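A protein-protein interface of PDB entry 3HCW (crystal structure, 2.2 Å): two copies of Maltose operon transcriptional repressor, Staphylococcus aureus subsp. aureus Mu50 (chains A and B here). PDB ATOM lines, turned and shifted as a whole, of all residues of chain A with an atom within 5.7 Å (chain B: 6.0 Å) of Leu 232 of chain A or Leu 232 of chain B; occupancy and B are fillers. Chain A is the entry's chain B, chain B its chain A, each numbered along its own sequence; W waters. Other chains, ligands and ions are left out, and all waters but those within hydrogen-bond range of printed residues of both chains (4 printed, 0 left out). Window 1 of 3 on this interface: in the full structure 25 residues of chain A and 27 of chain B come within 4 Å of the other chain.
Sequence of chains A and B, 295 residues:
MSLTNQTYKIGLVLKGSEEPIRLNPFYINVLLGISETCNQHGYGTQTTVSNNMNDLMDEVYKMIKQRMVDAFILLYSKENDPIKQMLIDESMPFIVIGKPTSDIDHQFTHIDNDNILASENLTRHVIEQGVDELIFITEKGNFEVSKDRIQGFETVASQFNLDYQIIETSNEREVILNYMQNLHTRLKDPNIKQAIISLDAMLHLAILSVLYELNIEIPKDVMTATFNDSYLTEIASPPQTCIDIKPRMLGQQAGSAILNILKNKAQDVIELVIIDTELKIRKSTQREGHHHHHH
Leu 23 of chain A touches Pro 25 of chain B (CD1 to CB, 3.6 Å).
Leu 23 of chain A touches Ser 230 of chain B (CD1 to CB, 3.8 Å).
Pro 25 of chain A touches Leu 23 of chain B.
Tyr 231 of chain B touches Met 202 of chain A.
Ile 235 of chain B touches Met 202 of chain A (CD1 to O, 3.7 Å).
Glu 19 of chain B touches Ser 230 of chain A.
Leu 232 of chain A touches Leu 232 of chain B (CD2 to CD1, 3.8 Å).
O of Met 202 of chain B touches CD1 of Ile 235 of chain A, at 3.9 Å.
Water W1 bridges the backbone carbonyl oxygen of Met 202 of chain A (2.6 Å) and the side-chain hydroxyl of Tyr 231 of chain B (2.7 Å).
Water W3 lies within hydrogen-bond range of O of Met 202 of chain B (2.7 Å) and OH of Tyr 231 of chain A (3.5 Å).
Water W2 lies within hydrogen-bond range of O of Leu 205 of chain A (2.7 Å), O of Ile 235 of chain B (2.7 Å) and OG of Ser 237 of chain B (2.9 Å).
Water W4 lies within hydrogen-bond range of the backbone carbonyl oxygen (O) of Ile 235 of chain A (2.9 Å) and the backbone carbonyl oxygen (O) of Leu 205 of chain B (2.9 Å).
The side-chain carboxylate of Glu 19 of chain B lies within hydrogen-bond range of the backbone NH of Tyr 231 of chain A (3.1 Å).
O of Leu 205 of chain A sits close to O of Ile 235 of chain B, 3.3 Å away.
The backbone carbonyl oxygen of Leu 205 of chain B lies close to the backbone carbonyl oxygen of Ile 235 of chain A (3.3 Å).
Leu 23 of chain A touches Ser 230 of chain B, but with the chains exchanged Ser 230 of chain A does not touch Leu 23 of chain B (4.5 Å).
Met 202 of chain A touches Tyr 231 of chain B, but with the chains exchanged Tyr 231 of chain A does not touch Met 202 of chain B (4.1 Å).
Met 202 of chain A touches Ile 235 of chain B, and with the chains exchanged Ile 235 of chain A touches Met 202 of chain B.
Leu 205 of chain A touches Ile 235 of chain B, and with the chains exchanged Ile 235 of chain A touches Leu 205 of chain B.
12 positions are printed for both chains.
Printed residues of chain A that touch a printed residue of chain B: Leu 23, Pro 25, Met 202, Leu 205, Ser 230, Tyr 231, Leu 232 and Ile 235.
Hydrophobic or aromatic side chains of chain A that line the printed part of chain B: Leu 23, Pro 25, Met 202, Leu 205, Tyr 231, Leu 232 and Ile 235.
Along chain A the printed residues that touch a printed residue of chain B span positions 23 to 235.
Along chain B the printed residues that touch a printed residue of chain A span positions 19 to 235.
Among the printed residues, 11 pairs touch across the chains.
Among the printed residues, no Asp or Glu carboxylate lies within 4 Å of a Lys or Arg side-chain nitrogen of the other chain.
The side-chain hydroxyl (OG) of Ser 230 of chain B lies close to the backbone NH (N) of Leu 232 of chain B, at 3.1 Å.
The backbone carbonyl oxygen (O) of Ser 230 of chain B sits at hydrogen-bond distance from the side-chain hydroxyl (OG1) of Thr 233 of chain B, at 3.0 Å.
OG of Ser 230 of chain A is in hydrogen-bond range of N of Leu 232 of chain A (3.1 Å).
The backbone carbonyl oxygen of Ser 230 of chain A sits at hydrogen-bond distance from the side-chain hydroxyl of Thr 233 of chain A (3.1 Å).
Of chain B, only Leu 232 comes within 4 Å of Leu 232 of chain A.
Leu 232 of chain B touches just one residue of chain A: Leu 232 (3.8 Å).
Of the printed residues of chain B, Leu 205 of chain A touches Ile 235.
Printed residues of chain B within 4 Å of Tyr 231 of chain A: Glu 19.
Printed residues of chain B within 4 Å of Ser 230 of chain A: Glu 19.
Ala 236 of chain A touches none of the printed residues of chain B.
The nearest printed residue of chain B that does not touch Ser 230 of chain A is Leu 23 of chain B (4.5 Å).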
ATOM      1  N   LEU A  23       5.592  14.324 -12.434  1.00  0.00           N
ATOM      2  CA  LEU A  23       4.986  14.072 -13.757  1.00  0.00           C
ATOM      3  C   LEU A  23       3.506  13.708 -13.681  1.00  0.00           C
ATOM      4  O   LEU A  23       2.846  13.576 -14.724  1.00  0.00           O
ATOM      5  CB  LEU A  23       5.731  12.983 -14.535  1.00  0.00           C
ATOM      6  CG  LEU A  23       7.221  13.167 -14.841  1.00  0.00           C
ATOM      7  CD1 LEU A  23       7.728  12.052 -15.746  1.00  0.00           C
ATOM      8  CD2 LEU A  23       7.536  14.530 -15.423  1.00  0.00           C
ATOM      9  N   ASN A  24       3.007  13.549 -12.450  1.00  0.00           N
ATOM     10  CA  ASN A  24       1.591  13.279 -12.177  1.00  0.00           C
ATOM     11  C   ASN A  24       0.788  14.530 -12.459  1.00  0.00           C
ATOM     12  O   ASN A  24       0.980  15.551 -11.792  1.00  0.00           O
ATOM     13  CB  ASN A  24       1.409  12.860 -10.714  1.00  0.00           C
ATOM     14  CG  ASN A  24       0.124  12.086 -10.464  1.00  0.00           C
ATOM     15  OD1 ASN A  24      -0.826  12.148 -11.238  1.00  0.00           O
ATOM     16  ND2 ASN A  24       0.099  11.342  -9.363  1.00  0.00           N
ATOM     17  N   PRO A  25      -0.113  14.460 -13.451  1.00  0.00           N
ATOM     18  CA  PRO A  25      -0.956  15.600 -13.826  1.00  0.00           C
ATOM     19  C   PRO A  25      -1.875  16.109 -12.710  1.00  0.00           C
ATOM     20  O   PRO A  25      -2.445  17.198 -12.852  1.00  0.00           O
ATOM     21  CB  PRO A  25      -1.795  15.051 -14.982  1.00  0.00           C
ATOM     22  CG  PRO A  25      -0.994  13.895 -15.517  1.00  0.00           C
ATOM     23  CD  PRO A  25      -0.381  13.284 -14.301  1.00  0.00           C
ATOM     24  N   ALA A 201      -4.120   7.055 -10.762  1.00  0.00           N
ATOM     25  CA  ALA A 201      -3.734   6.813 -12.158  1.00  0.00           C
ATOM     26  C   ALA A 201      -2.274   6.395 -12.384  1.00  0.00           C
ATOM     27  O   ALA A 201      -2.002   5.553 -13.236  1.00  0.00           O
ATOM     28  CB  ALA A 201      -4.069   8.026 -13.007  1.00  0.00           C
ATOM     29  N   MET A 202      -1.349   6.966 -11.613  1.00  0.00           N
ATOM     30  CA  MET A 202       0.073   6.685 -11.792  1.00  0.00           C
ATOM     31  C   MET A 202       0.445   5.266 -11.345  1.00  0.00           C
ATOM     32  O   MET A 202       1.158   4.576 -12.069  1.00  0.00           O
ATOM     33  CB  MET A 202       0.945   7.749 -11.105  1.00  0.00           C
ATOM     34  CG  MET A 202       2.398   7.781 -11.599  1.00  0.00           C
ATOM     35  SD  MET A 202       2.587   8.244 -13.344  1.00  0.00           S
ATOM     36  CE  MET A 202       2.379  10.004 -13.237  1.00  0.00           C
ATOM     37  N   LEU A 205      -1.101   2.663 -13.856  1.00  0.00           N
ATOM     38  CA  LEU A 205      -0.331   2.426 -15.072  1.00  0.00           C
ATOM     39  C   LEU A 205       0.703   1.326 -14.934  1.00  0.00           C
ATOM     40  O   LEU A 205       0.950   0.588 -15.882  1.00  0.00           O
ATOM     41  CB  LEU A 205       0.343   3.720 -15.549  1.00  0.00           C
ATOM     42  CG  LEU A 205      -0.571   4.798 -16.131  1.00  0.00           C
ATOM     43  CD1 LEU A 205       0.258   5.974 -16.609  1.00  0.00           C
ATOM     44  CD2 LEU A 205      -1.443   4.239 -17.249  1.00  0.00           C
ATOM     45  N   SER A 230      -6.838  12.126 -16.531  1.00  0.00           N
ATOM     46  CA  SER A 230      -5.949  12.987 -17.319  1.00  0.00           C
ATOM     47  C   SER A 230      -5.682  12.301 -18.641  1.00  0.00           C
ATOM     48  O   SER A 230      -6.335  11.311 -18.971  1.00  0.00           O
ATOM     49  CB  SER A 230      -4.623  13.264 -16.588  1.00  0.00           C
ATOM     50  OG  SER A 230      -3.749  12.150 -16.649  1.00  0.00           O
ATOM     51  N   TYR A 231      -4.716  12.825 -19.392  1.00  0.00           N
ATOM     52  CA  TYR A 231      -4.315  12.245 -20.672  1.00  0.00           C
ATOM     53  C   TYR A 231      -3.755  10.844 -20.454  1.00  0.00           C
ATOM     54  O   TYR A 231      -3.961   9.966 -21.274  1.00  0.00           O
ATOM     55  CB  TYR A 231      -3.292  13.150 -21.370  1.00  0.00           C
ATOM     56  CG  TYR A 231      -3.371  13.158 -22.884  1.00  0.00           C
ATOM     57  CD1 TYR A 231      -4.580  13.392 -23.547  1.00  0.00           C
ATOM     58  CD2 TYR A 231      -2.226  12.965 -23.657  1.00  0.00           C
ATOM     59  CE1 TYR A 231      -4.651  13.404 -24.943  1.00  0.00           C
ATOM     60  CE2 TYR A 231      -2.284  12.974 -25.049  1.00  0.00           C
ATOM     61  CZ  TYR A 231      -3.498  13.195 -25.686  1.00  0.00           C
ATOM     62  OH  TYR A 231      -3.550  13.206 -27.066  1.00  0.00           O
ATOM     63  N   LEU A 232      -3.096  10.630 -19.319  1.00  0.00           N
ATOM     64  CA  LEU A 232      -2.570   9.313 -18.945  1.00  0.00           C
ATOM     65  C   LEU A 232      -3.622   8.216 -18.795  1.00  0.00           C
ATOM     66  O   LEU A 232      -3.304   7.044 -18.972  1.00  0.00           O
ATOM     67  CB  LEU A 232      -1.743   9.398 -17.650  1.00  0.00           C
ATOM     68  CG  LEU A 232      -0.571  10.382 -17.560  1.00  0.00           C
ATOM     69  CD1 LEU A 232       0.197  10.106 -16.296  1.00  0.00           C
ATOM     70  CD2 LEU A 232       0.354  10.335 -18.779  1.00  0.00           C
ATOM     71  N   THR A 233      -4.855   8.573 -18.435  1.00  0.00           N
ATOM     72  CA  THR A 233      -5.927   7.578 -18.459  1.00  0.00           C
ATOM     73  C   THR A 233      -6.697   7.563 -19.782  1.00  0.00           C
ATOM     74  O   THR A 233      -7.201   6.516 -20.194  1.00  0.00           O
ATOM     75  CB  THR A 233      -6.894   7.678 -17.258  1.00  0.00           C
ATOM     76  OG1 THR A 233      -7.365   9.024 -17.103  1.00  0.00           O
ATOM     77  CG2 THR A 233      -6.209   7.215 -15.982  1.00  0.00           C
ATOM     78  N   GLU A 234      -6.775   8.713 -20.448  1.00  0.00           N
ATOM     79  CA  GLU A 234      -7.455   8.811 -21.741  1.00  0.00           C
ATOM     80  C   GLU A 234      -6.747   8.002 -22.833  1.00  0.00           C
ATOM     81  O   GLU A 234      -7.394   7.379 -23.682  1.00  0.00           O
ATOM     82  CB  GLU A 234      -7.593  10.277 -22.149  1.00  0.00           C
ATOM     83  CG  GLU A 234      -8.205  10.500 -23.526  1.00  0.00           C
ATOM     84  CD  GLU A 234      -8.715  11.905 -23.721  1.00  0.00           C
ATOM     85  OE1 GLU A 234      -9.673  12.076 -24.503  1.00  0.00           O
ATOM     86  OE2 GLU A 234      -8.166  12.835 -23.091  1.00  0.00           O
ATOM     87  N   ILE A 235      -5.417   8.004 -22.805  1.00  0.00           N
ATOM     88  CA  ILE A 235      -4.646   7.258 -23.793  1.00  0.00           C
ATOM     89  C   ILE A 235      -3.869   6.086 -23.206  1.00  0.00           C
ATOM     90  O   ILE A 235      -2.835   5.688 -23.757  1.00  0.00           O
ATOM     91  CB  ILE A 235      -3.719   8.170 -24.648  1.00  0.00           C
ATOM     92  CG1 ILE A 235      -2.752   8.971 -23.755  1.00  0.00           C
ATOM     93  CG2 ILE A 235      -4.571   9.047 -25.584  1.00  0.00           C
ATOM     94  CD1 ILE A 235      -1.503   9.415 -24.420  1.00  0.00           C
ATOM     95  N   ALA A 236      -4.373   5.534 -22.100  1.00  0.00           N
ATOM     96  CA  ALA A 236      -3.828   4.297 -21.509  1.00  0.00           C
ATOM     97  C   ALA A 236      -4.124   3.096 -22.410  1.00  0.00           C
ATOM     98  O   ALA A 236      -4.836   3.226 -23.412  1.00  0.00           O
ATOM     99  CB  ALA A 236      -4.397   4.065 -20.109  1.00  0.00           C
ATOM    100  N   GLU B  19      -2.672  20.400 -22.766  1.00  0.00           N
ATOM    101  CA  GLU B  19      -2.612  19.277 -21.825  1.00  0.00           C
ATOM    102  C   GLU B  19      -1.460  18.285 -22.104  1.00  0.00           C
ATOM    103  O   GLU B  19      -0.734  17.951 -21.179  1.00  0.00           O
ATOM    104  CB  GLU B  19      -3.971  18.560 -21.709  1.00  0.00           C
ATOM    105  CG  GLU B  19      -4.194  17.847 -20.373  1.00  0.00           C
ATOM    106  CD  GLU B  19      -5.074  16.600 -20.479  1.00  0.00           C
ATOM    107  OE1 GLU B  19      -5.611  16.322 -21.577  1.00  0.00           O
ATOM    108  OE2 GLU B  19      -5.220  15.893 -19.455  1.00  0.00           O
ATOM    109  N   LEU B  23       1.992  18.775 -19.501  1.00  0.00           N
ATOM    110  CA  LEU B  23       2.113  17.472 -18.831  1.00  0.00           C
ATOM    111  C   LEU B  23       3.229  16.652 -19.451  1.00  0.00           C
ATOM    112  O   LEU B  23       3.539  15.552 -18.961  1.00  0.00           O
ATOM    113  CB  LEU B  23       0.816  16.667 -18.937  1.00  0.00           C
ATOM    114  CG  LEU B  23      -0.391  16.781 -17.993  1.00  0.00           C
ATOM    115  CD1 LEU B  23      -0.879  18.212 -17.759  1.00  0.00           C
ATOM    116  CD2 LEU B  23      -1.517  15.922 -18.563  1.00  0.00           C
ATOM    117  N   PRO B  25       6.645  15.376 -19.897  1.00  0.00           N
ATOM    118  CA  PRO B  25       7.813  15.231 -19.025  1.00  0.00           C
ATOM    119  C   PRO B  25       9.091  15.858 -19.580  1.00  0.00           C
ATOM    120  O   PRO B  25      10.060  16.014 -18.838  1.00  0.00           O
ATOM    121  CB  PRO B  25       8.003  13.709 -18.938  1.00  0.00           C
ATOM    122  CG  PRO B  25       6.671  13.147 -19.222  1.00  0.00           C
ATOM    123  CD  PRO B  25       6.106  14.061 -20.283  1.00  0.00           C
ATOM    124  N   ALA B 201       7.605  10.465 -26.661  1.00  0.00           N
ATOM    125  CA  ALA B 201       6.878   9.555 -25.778  1.00  0.00           C
ATOM    126  C   ALA B 201       5.375   9.839 -25.624  1.00  0.00           C
ATOM    127  O   ALA B 201       4.590   8.912 -25.514  1.00  0.00           O
ATOM    128  CB  ALA B 201       7.548   9.548 -24.409  1.00  0.00           C
ATOM    129  N   MET B 202       4.982  11.114 -25.617  1.00  0.00           N
ATOM    130  CA  MET B 202       3.569  11.491 -25.461  1.00  0.00           C
ATOM    131  C   MET B 202       2.740  11.035 -26.661  1.00  0.00           C
ATOM    132  O   MET B 202       1.672  10.442 -26.492  1.00  0.00           O
ATOM    133  CB  MET B 202       3.434  13.005 -25.217  1.00  0.00           C
ATOM    134  CG  MET B 202       2.158  13.424 -24.470  1.00  0.00           C
ATOM    135  SD  MET B 202       1.777  12.502 -22.944  1.00  0.00           S
ATOM    136  CE  MET B 202       3.248  12.806 -21.975  1.00  0.00           C
ATOM    137  N   LEU B 205       2.586   7.058 -26.619  1.00  0.00           N
ATOM    138  CA  LEU B 205       1.589   6.470 -25.727  1.00  0.00           C
ATOM    139  C   LEU B 205       0.211   6.348 -26.386  1.00  0.00           C
ATOM    140  O   LEU B 205      -0.517   5.403 -26.108  1.00  0.00           O
ATOM    141  CB  LEU B 205       1.481   7.247 -24.427  1.00  0.00           C
ATOM    142  CG  LEU B 205       2.645   7.213 -23.422  1.00  0.00           C
ATOM    143  CD1 LEU B 205       2.337   8.179 -22.288  1.00  0.00           C
ATOM    144  CD2 LEU B 205       2.920   5.822 -22.868  1.00  0.00           C
ATOM    145  N   SER B 230      11.189   8.697 -19.673  1.00  0.00           N
ATOM    146  CA  SER B 230      10.767   9.120 -18.355  1.00  0.00           C
ATOM    147  C   SER B 230      10.143   7.904 -17.688  1.00  0.00           C
ATOM    148  O   SER B 230      10.197   6.790 -18.222  1.00  0.00           O
ATOM    149  CB  SER B 230       9.731  10.243 -18.461  1.00  0.00           C
ATOM    150  OG  SER B 230       8.510   9.748 -18.993  1.00  0.00           O
ATOM    151  N   TYR B 231       9.517   8.144 -16.543  1.00  0.00           N
ATOM    152  CA  TYR B 231       8.771   7.134 -15.817  1.00  0.00           C
ATOM    153  C   TYR B 231       7.642   6.548 -16.661  1.00  0.00           C
ATOM    154  O   TYR B 231       7.285   5.386 -16.488  1.00  0.00           O
ATOM    155  CB  TYR B 231       8.235   7.719 -14.497  1.00  0.00           C
ATOM    156  CG  TYR B 231       7.658   6.690 -13.549  1.00  0.00           C
ATOM    157  CD1 TYR B 231       8.449   5.653 -13.034  1.00  0.00           C
ATOM    158  CD2 TYR B 231       6.324   6.752 -13.163  1.00  0.00           C
ATOM    159  CE1 TYR B 231       7.915   4.699 -12.161  1.00  0.00           C
ATOM    160  CE2 TYR B 231       5.779   5.810 -12.288  1.00  0.00           C
ATOM    161  CZ  TYR B 231       6.571   4.788 -11.795  1.00  0.00           C
ATOM    162  OH  TYR B 231       6.008   3.864 -10.939  1.00  0.00           O
ATOM    163  N   LEU B 232       7.128   7.336 -17.606  1.00  0.00           N
ATOM    164  CA  LEU B 232       5.971   6.945 -18.421  1.00  0.00           C
ATOM    165  C   LEU B 232       6.254   5.893 -19.482  1.00  0.00           C
ATOM    166  O   LEU B 232       5.395   5.068 -19.767  1.00  0.00           O
ATOM    167  CB  LEU B 232       5.320   8.176 -19.058  1.00  0.00           C
ATOM    168  CG  LEU B 232       4.693   9.166 -18.071  1.00  0.00           C
ATOM    169  CD1 LEU B 232       4.196  10.400 -18.801  1.00  0.00           C
ATOM    170  CD2 LEU B 232       3.564   8.513 -17.263  1.00  0.00           C
ATOM    171  N   THR B 233       7.445   5.930 -20.076  1.00  0.00           N
ATOM    172  CA  THR B 233       7.856   4.891 -21.012  1.00  0.00           C
ATOM    173  C   THR B 233       8.293   3.636 -20.257  1.00  0.00           C
ATOM    174  O   THR B 233       8.090   2.529 -20.735  1.00  0.00           O
ATOM    175  CB  THR B 233       8.989   5.357 -21.933  1.00  0.00           C
ATOM    176  OG1 THR B 233       9.963   6.076 -21.171  1.00  0.00           O
ATOM    177  CG2 THR B 233       8.455   6.260 -23.031  1.00  0.00           C
ATOM    178  N   GLU B 234       8.888   3.830 -19.078  1.00  0.00           N
ATOM    179  CA  GLU B 234       9.238   2.745 -18.169  1.00  0.00           C
ATOM    180  C   GLU B 234       8.035   1.882 -17.762  1.00  0.00           C
ATOM    181  O   GLU B 234       8.145   0.667 -17.671  1.00  0.00           O
ATOM    182  CB  GLU B 234       9.908   3.315 -16.915  1.00  0.00           C
ATOM    183  CG  GLU B 234      10.530   2.248 -16.015  1.00  0.00           C
ATOM    184  CD  GLU B 234      11.280   2.816 -14.815  1.00  0.00           C
ATOM    185  OE1 GLU B 234      11.338   2.110 -13.789  1.00  0.00           O
ATOM    186  OE2 GLU B 234      11.813   3.949 -14.895  1.00  0.00           O
ATOM    187  N   ILE B 235       6.889   2.511 -17.516  1.00  0.00           N
ATOM    188  CA  ILE B 235       5.703   1.761 -17.091  1.00  0.00           C
ATOM    189  C   ILE B 235       4.579   1.782 -18.137  1.00  0.00           C
ATOM    190  O   ILE B 235       3.409   1.583 -17.808  1.00  0.00           O
ATOM    191  CB  ILE B 235       5.201   2.169 -15.668  1.00  0.00           C
ATOM    192  CG1 ILE B 235       4.760   3.641 -15.630  1.00  0.00           C
ATOM    193  CG2 ILE B 235       6.293   1.886 -14.608  1.00  0.00           C
ATOM    194  CD1 ILE B 235       3.836   3.979 -14.478  1.00  0.00           C
ATOM    195  N   ALA B 236       4.957   1.989 -19.401  1.00  0.00           N
ATOM    196  CA  ALA B 236       4.039   1.822 -20.533  1.00  0.00           C
ATOM    197  C   ALA B 236       3.705   0.343 -20.714  1.00  0.00           C
ATOM    198  O   ALA B 236       4.313  -0.512 -20.079  1.00  0.00           O
ATOM    199  CB  ALA B 236       4.652   2.386 -21.809  1.00  0.00           C
ATOM    200  N   SER B 237       2.735   0.058 -21.577  1.00  0.00           N
ATOM    201  CA  SER B 237       2.314  -1.294 -21.891  1.00  0.00           C
ATOM    202  C   SER B 237       2.714  -1.622 -23.333  1.00  0.00           C
ATOM    203  O   SER B 237       2.041  -1.175 -24.269  1.00  0.00           O
ATOM    204  CB  SER B 237       0.790  -1.438 -21.723  1.00  0.00           C
ATOM    205  OG  SER B 237       0.388  -1.200 -20.373  1.00  0.00           O
HETATM  206  O   HOH W   1       3.347   3.943 -10.724  1.00  0.00           O
HETATM  207  O   HOH W   2       0.846   1.009 -18.565  1.00  0.00           O
HETATM  208  O   HOH W   3      -0.367  11.912 -27.423  1.00  0.00           O
HETATM  209  O   HOH W   4      -0.865   3.584 -23.831  1.00  0.00           O
